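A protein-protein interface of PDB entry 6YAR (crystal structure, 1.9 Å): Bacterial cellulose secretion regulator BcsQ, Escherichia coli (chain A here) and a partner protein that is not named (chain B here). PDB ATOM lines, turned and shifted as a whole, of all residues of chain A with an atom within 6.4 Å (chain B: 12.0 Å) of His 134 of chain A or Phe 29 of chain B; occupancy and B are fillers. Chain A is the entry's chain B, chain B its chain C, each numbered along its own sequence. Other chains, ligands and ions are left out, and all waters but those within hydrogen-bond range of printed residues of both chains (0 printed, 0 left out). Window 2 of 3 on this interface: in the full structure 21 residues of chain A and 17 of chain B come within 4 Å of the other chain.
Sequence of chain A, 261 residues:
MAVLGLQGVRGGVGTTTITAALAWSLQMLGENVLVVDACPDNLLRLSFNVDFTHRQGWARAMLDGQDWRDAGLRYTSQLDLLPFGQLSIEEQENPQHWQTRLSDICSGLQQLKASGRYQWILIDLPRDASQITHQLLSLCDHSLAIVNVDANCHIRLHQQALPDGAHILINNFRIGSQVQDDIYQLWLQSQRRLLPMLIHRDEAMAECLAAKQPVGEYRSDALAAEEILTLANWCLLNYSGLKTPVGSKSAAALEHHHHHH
The side-chain hydroxyl of Ser 30 of chain B lies within hydrogen-bond range of the side-chain carboxylate of Asp 164 of chain A, at 3.4 Å. O of Ser 30 of chain B is in hydrogen-bond range of N of Leu 162 of chain A, 2.8 Å away.
The backbone carbonyl oxygen (O) of Ala 129 of chain A lies within hydrogen-bond range of a ring nitrogen (NE2) of His 134 of chain A. The backbone carbonyl oxygen (O) of Ala 161 of chain A is in hydrogen-bond range of the guanidinium group (NH2) of Arg 127 of chain A (2.9 Å).
Among the printed residues, merely in contact across the chains: His 134 of chain A with Phe 29 of chain B, Ala 161 of chain A with Ser 30 of chain B, Leu 137 of chain A with Phe 29 of chain B, Leu 162 of chain A with Phe 29 of chain B, Leu 162 of chain A with Pro 32 of chain B and Ala 161 of chain A with Phe 29 of chain B.
His 134 of chain A touches one residue of chain B. Phe 29 of chain B touches four residues of chain A. Ala 129 of chain A touches none of the printed residues of chain B. No residue of chain B comes within 4 Å of Ile 132 of chain A. No residue of chain B comes within 4 Å of Thr 133 of chain A. No residue of chain B comes within 4 Å of Gln 135 of chain A. No residue of chain B comes within 4 Å of Leu 136 of chain A. Leu 137 of chain A touches just one residue of chain B: Phe 29 (3.5 Å). Of chain B, only Phe 29 (3.7 Å) and Ser 30 (3.3 Å) come within 4 Å of Ala 161 of chain A. Pro 163 of chain A touches none of the printed residues of chain B. Asp 164 of chain A touches just one residue of chain B: Ser 30 (3.4 Å). Of the printed residues of chain B, Leu 162 of chain A touches Phe 29 (3.5 Å), Ser 30 (2.8 Å) and Pro 32 (3.6 Å). Printed residues of chain A within 4 Å of Pro 32 of chain B: Leu 162. Asp 128 of chain A touches none of the printed residues of chain B. Arg 127 of chain A touches none of the printed residues of chain B. The nearest residue of chain A that does not touch Phe 29 of chain B is Asp 164 of chain A (4.1 Å). The nearest printed residue of chain B that does not touch Leu 162 of chain A is Leu 31 of chain B (4.9 Å).
Hydrophobic or aromatic side chains of chain A that line the printed part of chain B: His 134, Leu 137, Ala 161 and Leu 162. Hydrophobic or aromatic side chains of chain B within 4 Å of the printed part of chain A: Phe 29 and Pro 32. Among the printed residues, 8 pairs touch across the chains.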
ATOM      1  N   GLN A   7      -9.569 -27.076 -19.856  1.00  0.00           N
ATOM      2  CA  GLN A   7      -9.715 -26.000 -18.879  1.00  0.00           C
ATOM      3  C   GLN A   7      -9.057 -26.427 -17.572  1.00  0.00           C
ATOM      4  O   GLN A   7      -9.398 -27.475 -17.013  1.00  0.00           O
ATOM      5  CB  GLN A   7     -11.194 -25.662 -18.662  1.00  0.00           C
ATOM      6  CG  GLN A   7     -11.435 -24.452 -17.736  1.00  0.00           C
ATOM      7  CD  GLN A   7     -12.899 -24.261 -17.388  1.00  0.00           C
ATOM      8  OE1 GLN A   7     -13.551 -25.180 -16.889  1.00  0.00           O
ATOM      9  NE2 GLN A   7     -13.426 -23.054 -17.643  1.00  0.00           N
ATOM     10  N   ARG A 127      -9.972 -20.029 -16.878  1.00  0.00           N
ATOM     11  CA  ARG A 127     -10.709 -20.363 -15.666  1.00  0.00           C
ATOM     12  C   ARG A 127     -11.344 -19.091 -15.116  1.00  0.00           C
ATOM     13  O   ARG A 127     -10.981 -18.575 -14.064  1.00  0.00           O
ATOM     14  CB  ARG A 127      -9.793 -21.036 -14.644  1.00  0.00           C
ATOM     15  CG  ARG A 127     -10.542 -21.652 -13.454  1.00  0.00           C
ATOM     16  CD  ARG A 127     -11.440 -22.805 -13.904  1.00  0.00           C
ATOM     17  NE  ARG A 127     -12.650 -22.927 -13.099  1.00  0.00           N
ATOM     18  CZ  ARG A 127     -13.343 -24.053 -12.946  1.00  0.00           C
ATOM     19  NH1 ARG A 127     -12.936 -25.183 -13.525  1.00  0.00           N
ATOM     20  NH2 ARG A 127     -14.440 -24.056 -12.193  1.00  0.00           N
ATOM     21  N   ASP A 128     -12.282 -18.562 -15.897  1.00  0.00           N
ATOM     22  CA  ASP A 128     -13.175 -17.506 -15.456  1.00  0.00           C
ATOM     23  C   ASP A 128     -14.607 -17.973 -15.658  1.00  0.00           C
ATOM     24  O   ASP A 128     -14.868 -19.003 -16.283  1.00  0.00           O
ATOM     25  CB  ASP A 128     -12.926 -16.165 -16.178  1.00  0.00           C
ATOM     26  CG  ASP A 128     -12.998 -16.269 -17.694  1.00  0.00           C
ATOM     27  OD1 ASP A 128     -13.927 -16.915 -18.225  1.00  0.00           O
ATOM     28  OD2 ASP A 128     -12.135 -15.661 -18.366  1.00  0.00           O
ATOM     29  N   ALA A 129     -15.535 -17.213 -15.103  1.00  0.00           N
ATOM     30  CA  ALA A 129     -16.951 -17.532 -15.173  1.00  0.00           C
ATOM     31  C   ALA A 129     -17.688 -16.602 -16.130  1.00  0.00           C
ATOM     32  O   ALA A 129     -18.864 -16.305 -15.925  1.00  0.00           O
ATOM     33  CB  ALA A 129     -17.576 -17.470 -13.780  1.00  0.00           C
ATOM     34  N   SER A 130     -17.005 -16.128 -17.171  1.00  0.00           N
ATOM     35  CA  SER A 130     -17.637 -15.239 -18.132  1.00  0.00           C
ATOM     36  C   SER A 130     -18.661 -15.997 -18.966  1.00  0.00           C
ATOM     37  O   SER A 130     -18.584 -17.218 -19.129  1.00  0.00           O
ATOM     38  CB  SER A 130     -16.593 -14.589 -19.039  1.00  0.00           C
ATOM     39  OG  SER A 130     -15.957 -15.542 -19.864  1.00  0.00           O
ATOM     40  N   GLN A 131     -19.643 -15.257 -19.485  1.00  0.00           N
ATOM     41  CA  GLN A 131     -20.675 -15.880 -20.304  1.00  0.00           C
ATOM     42  C   GLN A 131     -20.084 -16.527 -21.543  1.00  0.00           C
ATOM     43  O   GLN A 131     -20.594 -17.551 -22.008  1.00  0.00           O
ATOM     44  CB  GLN A 131     -21.730 -14.848 -20.701  1.00  0.00           C
ATOM     45  CG  GLN A 131     -21.192 -13.690 -21.529  1.00  0.00           C
ATOM     46  CD  GLN A 131     -22.299 -12.766 -22.036  1.00  0.00           C
ATOM     47  OE1 GLN A 131     -22.971 -12.096 -21.253  1.00  0.00           O
ATOM     48  NE2 GLN A 131     -22.487 -12.731 -23.351  1.00  0.00           N
ATOM     49  N   ILE A 132     -19.007 -15.954 -22.082  1.00  0.00           N
ATOM     50  CA  ILE A 132     -18.402 -16.506 -23.288  1.00  0.00           C
ATOM     51  C   ILE A 132     -17.690 -17.818 -22.978  1.00  0.00           C
ATOM     52  O   ILE A 132     -17.769 -18.775 -23.759  1.00  0.00           O
ATOM     53  CB  ILE A 132     -17.464 -15.470 -23.937  1.00  0.00           C
ATOM     54  CG1 ILE A 132     -16.423 -16.162 -24.820  1.00  0.00           C
ATOM     55  CG2 ILE A 132     -16.820 -14.584 -22.884  1.00  0.00           C
ATOM     56  CD1 ILE A 132     -15.660 -15.213 -25.696  1.00  0.00           C
ATOM     57  N   THR A 133     -17.001 -17.900 -21.834  1.00  0.00           N
ATOM     58  CA  THR A 133     -16.436 -19.186 -21.440  1.00  0.00           C
ATOM     59  C   THR A 133     -17.536 -20.228 -21.284  1.00  0.00           C
ATOM     60  O   THR A 133     -17.390 -21.369 -21.740  1.00  0.00           O
ATOM     61  CB  THR A 133     -15.634 -19.059 -20.139  1.00  0.00           C
ATOM     62  OG1 THR A 133     -14.509 -18.197 -20.342  1.00  0.00           O
ATOM     63  CG2 THR A 133     -15.132 -20.424 -19.693  1.00  0.00           C
ATOM     64  N   HIS A 134     -18.651 -19.844 -20.659  1.00  0.00           N
ATOM     65  CA  HIS A 134     -19.780 -20.759 -20.522  1.00  0.00           C
ATOM     66  C   HIS A 134     -20.296 -21.207 -21.885  1.00  0.00           C
ATOM     67  O   HIS A 134     -20.573 -22.394 -22.093  1.00  0.00           O
ATOM     68  CB  HIS A 134     -20.906 -20.095 -19.732  1.00  0.00           C
ATOM     69  CG  HIS A 134     -20.570 -19.806 -18.303  1.00  0.00           C
ATOM     70  ND1 HIS A 134     -19.478 -20.355 -17.667  1.00  0.00           N
ATOM     71  CD2 HIS A 134     -21.189 -19.026 -17.382  1.00  0.00           C
ATOM     72  CE1 HIS A 134     -19.439 -19.929 -16.415  1.00  0.00           C
ATOM     73  NE2 HIS A 134     -20.465 -19.120 -16.218  1.00  0.00           N
ATOM     74  N   GLN A 135     -20.428 -20.272 -22.828  1.00  0.00           N
ATOM     75  CA  GLN A 135     -21.017 -20.607 -24.121  1.00  0.00           C
ATOM     76  C   GLN A 135     -20.057 -21.431 -24.978  1.00  0.00           C
ATOM     77  O   GLN A 135     -20.485 -22.342 -25.698  1.00  0.00           O
ATOM     78  CB  GLN A 135     -21.448 -19.332 -24.844  1.00  0.00           C
ATOM     79  CG  GLN A 135     -22.666 -18.637 -24.234  1.00  0.00           C
ATOM     80  CD  GLN A 135     -22.880 -17.228 -24.779  1.00  0.00           C
ATOM     81  OE1 GLN A 135     -22.019 -16.682 -25.474  1.00  0.00           O
ATOM     82  NE2 GLN A 135     -24.032 -16.633 -24.465  1.00  0.00           N
ATOM     83  N   LEU A 136     -18.755 -21.134 -24.917  1.00  0.00           N
ATOM     84  CA  LEU A 136     -17.794 -21.985 -25.617  1.00  0.00           C
ATOM     85  C   LEU A 136     -17.820 -23.401 -25.063  1.00  0.00           C
ATOM     86  O   LEU A 136     -17.752 -24.374 -25.822  1.00  0.00           O
ATOM     87  CB  LEU A 136     -16.388 -21.391 -25.532  1.00  0.00           C
ATOM     88  CG  LEU A 136     -16.220 -20.136 -26.394  1.00  0.00           C
ATOM     89  CD1 LEU A 136     -14.843 -19.509 -26.206  1.00  0.00           C
ATOM     90  CD2 LEU A 136     -16.503 -20.440 -27.879  1.00  0.00           C
ATOM     91  N   LEU A 137     -17.924 -23.537 -23.739  1.00  0.00           N
ATOM     92  CA  LEU A 137     -18.043 -24.865 -23.145  1.00  0.00           C
ATOM     93  C   LEU A 137     -19.286 -25.586 -23.638  1.00  0.00           C
ATOM     94  O   LEU A 137     -19.269 -26.813 -23.795  1.00  0.00           O
ATOM     95  CB  LEU A 137     -18.063 -24.763 -21.618  1.00  0.00           C
ATOM     96  CG  LEU A 137     -16.718 -24.938 -20.921  1.00  0.00           C
ATOM     97  CD1 LEU A 137     -16.857 -24.679 -19.431  1.00  0.00           C
ATOM     98  CD2 LEU A 137     -16.168 -26.344 -21.191  1.00  0.00           C
ATOM     99  N   SER A 138     -20.368 -24.848 -23.897  1.00  0.00           N
ATOM    100  CA  SER A 138     -21.605 -25.487 -24.331  1.00  0.00           C
ATOM    101  C   SER A 138     -21.507 -26.082 -25.735  1.00  0.00           C
ATOM    102  O   SER A 138     -22.273 -26.997 -26.054  1.00  0.00           O
ATOM    103  CB  SER A 138     -22.768 -24.499 -24.264  1.00  0.00           C
ATOM    104  OG  SER A 138     -22.524 -23.369 -25.080  1.00  0.00           O
ATOM    105  N   LEU A 139     -20.593 -25.608 -26.576  1.00  0.00           N
ATOM    106  CA  LEU A 139     -20.443 -26.211 -27.896  1.00  0.00           C
ATOM    107  C   LEU A 139     -19.368 -27.286 -27.933  1.00  0.00           C
ATOM    108  O   LEU A 139     -19.181 -27.915 -28.985  1.00  0.00           O
ATOM    109  CB  LEU A 139     -20.163 -25.145 -28.965  1.00  0.00           C
ATOM    110  CG  LEU A 139     -19.101 -24.053 -28.847  1.00  0.00           C
ATOM    111  CD1 LEU A 139     -17.759 -24.539 -29.329  1.00  0.00           C
ATOM    112  CD2 LEU A 139     -19.559 -22.818 -29.649  1.00  0.00           C
ATOM    113  N   ALA A 161     -17.478 -26.151  -9.585  1.00  0.00           N
ATOM    114  CA  ALA A 161     -18.064 -26.928 -10.663  1.00  0.00           C
ATOM    115  C   ALA A 161     -17.049 -27.147 -11.773  1.00  0.00           C
ATOM    116  O   ALA A 161     -16.259 -26.255 -12.103  1.00  0.00           O
ATOM    117  CB  ALA A 161     -19.305 -26.231 -11.226  1.00  0.00           C
ATOM    118  N   LEU A 162     -17.071 -28.344 -12.337  1.00  0.00           N
ATOM    119  CA  LEU A 162     -16.362 -28.682 -13.554  1.00  0.00           C
ATOM    120  C   LEU A 162     -17.333 -28.711 -14.727  1.00  0.00           C
ATOM    121  O   LEU A 162     -18.545 -28.856 -14.537  1.00  0.00           O
ATOM    122  CB  LEU A 162     -15.681 -30.050 -13.418  1.00  0.00           C
ATOM    123  CG  LEU A 162     -14.544 -30.204 -12.409  1.00  0.00           C
ATOM    124  CD1 LEU A 162     -13.823 -31.524 -12.628  1.00  0.00           C
ATOM    125  CD2 LEU A 162     -13.575 -29.040 -12.491  1.00  0.00           C
ATOM    126  N   PRO A 163     -16.840 -28.565 -15.957  1.00  0.00           N
ATOM    127  CA  PRO A 163     -17.723 -28.720 -17.114  1.00  0.00           C
ATOM    128  C   PRO A 163     -18.410 -30.075 -17.069  1.00  0.00           C
ATOM    129  O   PRO A 163     -17.802 -31.087 -16.712  1.00  0.00           O
ATOM    130  CB  PRO A 163     -16.768 -28.600 -18.304  1.00  0.00           C
ATOM    131  CG  PRO A 163     -15.652 -27.756 -17.791  1.00  0.00           C
ATOM    132  CD  PRO A 163     -15.472 -28.195 -16.364  1.00  0.00           C
ATOM    133  N   ASP A 164     -19.699 -30.082 -17.390  1.00  0.00           N
ATOM    134  CA  ASP A 164     -20.471 -31.311 -17.289  1.00  0.00           C
ATOM    135  C   ASP A 164     -19.885 -32.376 -18.206  1.00  0.00           C
ATOM    136  O   ASP A 164     -19.572 -32.110 -19.370  1.00  0.00           O
ATOM    137  CB  ASP A 164     -21.935 -31.055 -17.636  1.00  0.00           C
ATOM    138  CG  ASP A 164     -22.842 -32.165 -17.152  1.00  0.00           C
ATOM    139  OD1 ASP A 164     -23.115 -32.211 -15.931  1.00  0.00           O
ATOM    140  OD2 ASP A 164     -23.268 -32.991 -17.989  1.00  0.00           O
ATOM    141  N   PHE B  29     -22.489 -27.414 -15.769  1.00  0.00           N
ATOM    142  CA  PHE B  29     -21.612 -27.259 -14.609  1.00  0.00           C
ATOM    143  C   PHE B  29     -22.136 -28.002 -13.391  1.00  0.00           C
ATOM    144  O   PHE B  29     -23.236 -27.729 -12.913  1.00  0.00           O
ATOM    145  CB  PHE B  29     -21.436 -25.785 -14.253  1.00  0.00           C
ATOM    146  CG  PHE B  29     -20.894 -24.959 -15.370  1.00  0.00           C
ATOM    147  CD1 PHE B  29     -19.583 -25.110 -15.782  1.00  0.00           C
ATOM    148  CD2 PHE B  29     -21.693 -24.024 -16.007  1.00  0.00           C
ATOM    149  CE1 PHE B  29     -19.080 -24.348 -16.812  1.00  0.00           C
ATOM    150  CE2 PHE B  29     -21.195 -23.260 -17.039  1.00  0.00           C
ATOM    151  CZ  PHE B  29     -19.886 -23.423 -17.444  1.00  0.00           C
ATOM    152  N   SER B  30     -21.333 -28.934 -12.884  1.00  0.00           N
ATOM    153  CA  SER B  30     -21.678 -29.680 -11.686  1.00  0.00           C
ATOM    154  C   SER B  30     -20.413 -29.946 -10.880  1.00  0.00           C
ATOM    155  O   SER B  30     -19.292 -29.849 -11.389  1.00  0.00           O
ATOM    156  CB  SER B  30     -22.394 -30.998 -12.024  1.00  0.00           C
ATOM    157  OG  SER B  30     -21.641 -31.778 -12.939  1.00  0.00           O
ATOM    158  N   LEU B  31     -20.610 -30.271  -9.606  1.00  0.00           N
ATOM    159  CA  LEU B  31     -19.483 -30.604  -8.749  1.00  0.00           C
ATOM    160  C   LEU B  31     -18.940 -31.982  -9.123  1.00  0.00           C
ATOM    161  O   LEU B  31     -19.708 -32.870  -9.506  1.00  0.00           O
ATOM    162  CB  LEU B  31     -19.894 -30.578  -7.274  1.00  0.00           C
ATOM    163  CG  LEU B  31     -20.416 -29.251  -6.708  1.00  0.00           C
ATOM    164  CD1 LEU B  31     -21.925 -29.123  -6.894  1.00  0.00           C
ATOM    165  CD2 LEU B  31     -20.036 -29.100  -5.242  1.00  0.00           C
ATOM    166  N   PRO B  32     -17.624 -32.182  -9.034  1.00  0.00           N
ATOM    167  CA  PRO B  32     -17.032 -33.459  -9.459  1.00  0.00           C
ATOM    168  C   PRO B  32     -17.610 -34.655  -8.713  1.00  0.00           C
ATOM    169  O   PRO B  32     -17.881 -34.599  -7.512  1.00  0.00           O
ATOM    170  CB  PRO B  32     -15.543 -33.272  -9.146  1.00  0.00           C
ATOM    171  CG  PRO B  32     -15.339 -31.795  -9.236  1.00  0.00           C
ATOM    172  CD  PRO B  32     -16.597 -31.182  -8.699  1.00  0.00           C
ATOM    173  N   ASP B  33     -17.798 -35.748  -9.448  1.00  0.00           N
ATOM    174  CA  ASP B  33     -18.289 -36.989  -8.860  1.00  0.00           C
ATOM    175  C   ASP B  33     -17.187 -37.592  -7.995  1.00  0.00           C
ATOM    176  O   ASP B  33     -16.178 -38.083  -8.512  1.00  0.00           O
ATOM    177  CB  ASP B  33     -18.726 -37.949  -9.964  1.00  0.00           C
ATOM    178  CG  ASP B  33     -19.438 -39.180  -9.428  1.00  0.00           C
ATOM    179  OD1 ASP B  33     -19.786 -39.206  -8.226  1.00  0.00           O
ATOM    180  OD2 ASP B  33     -19.642 -40.129 -10.209  1.00  0.00           O
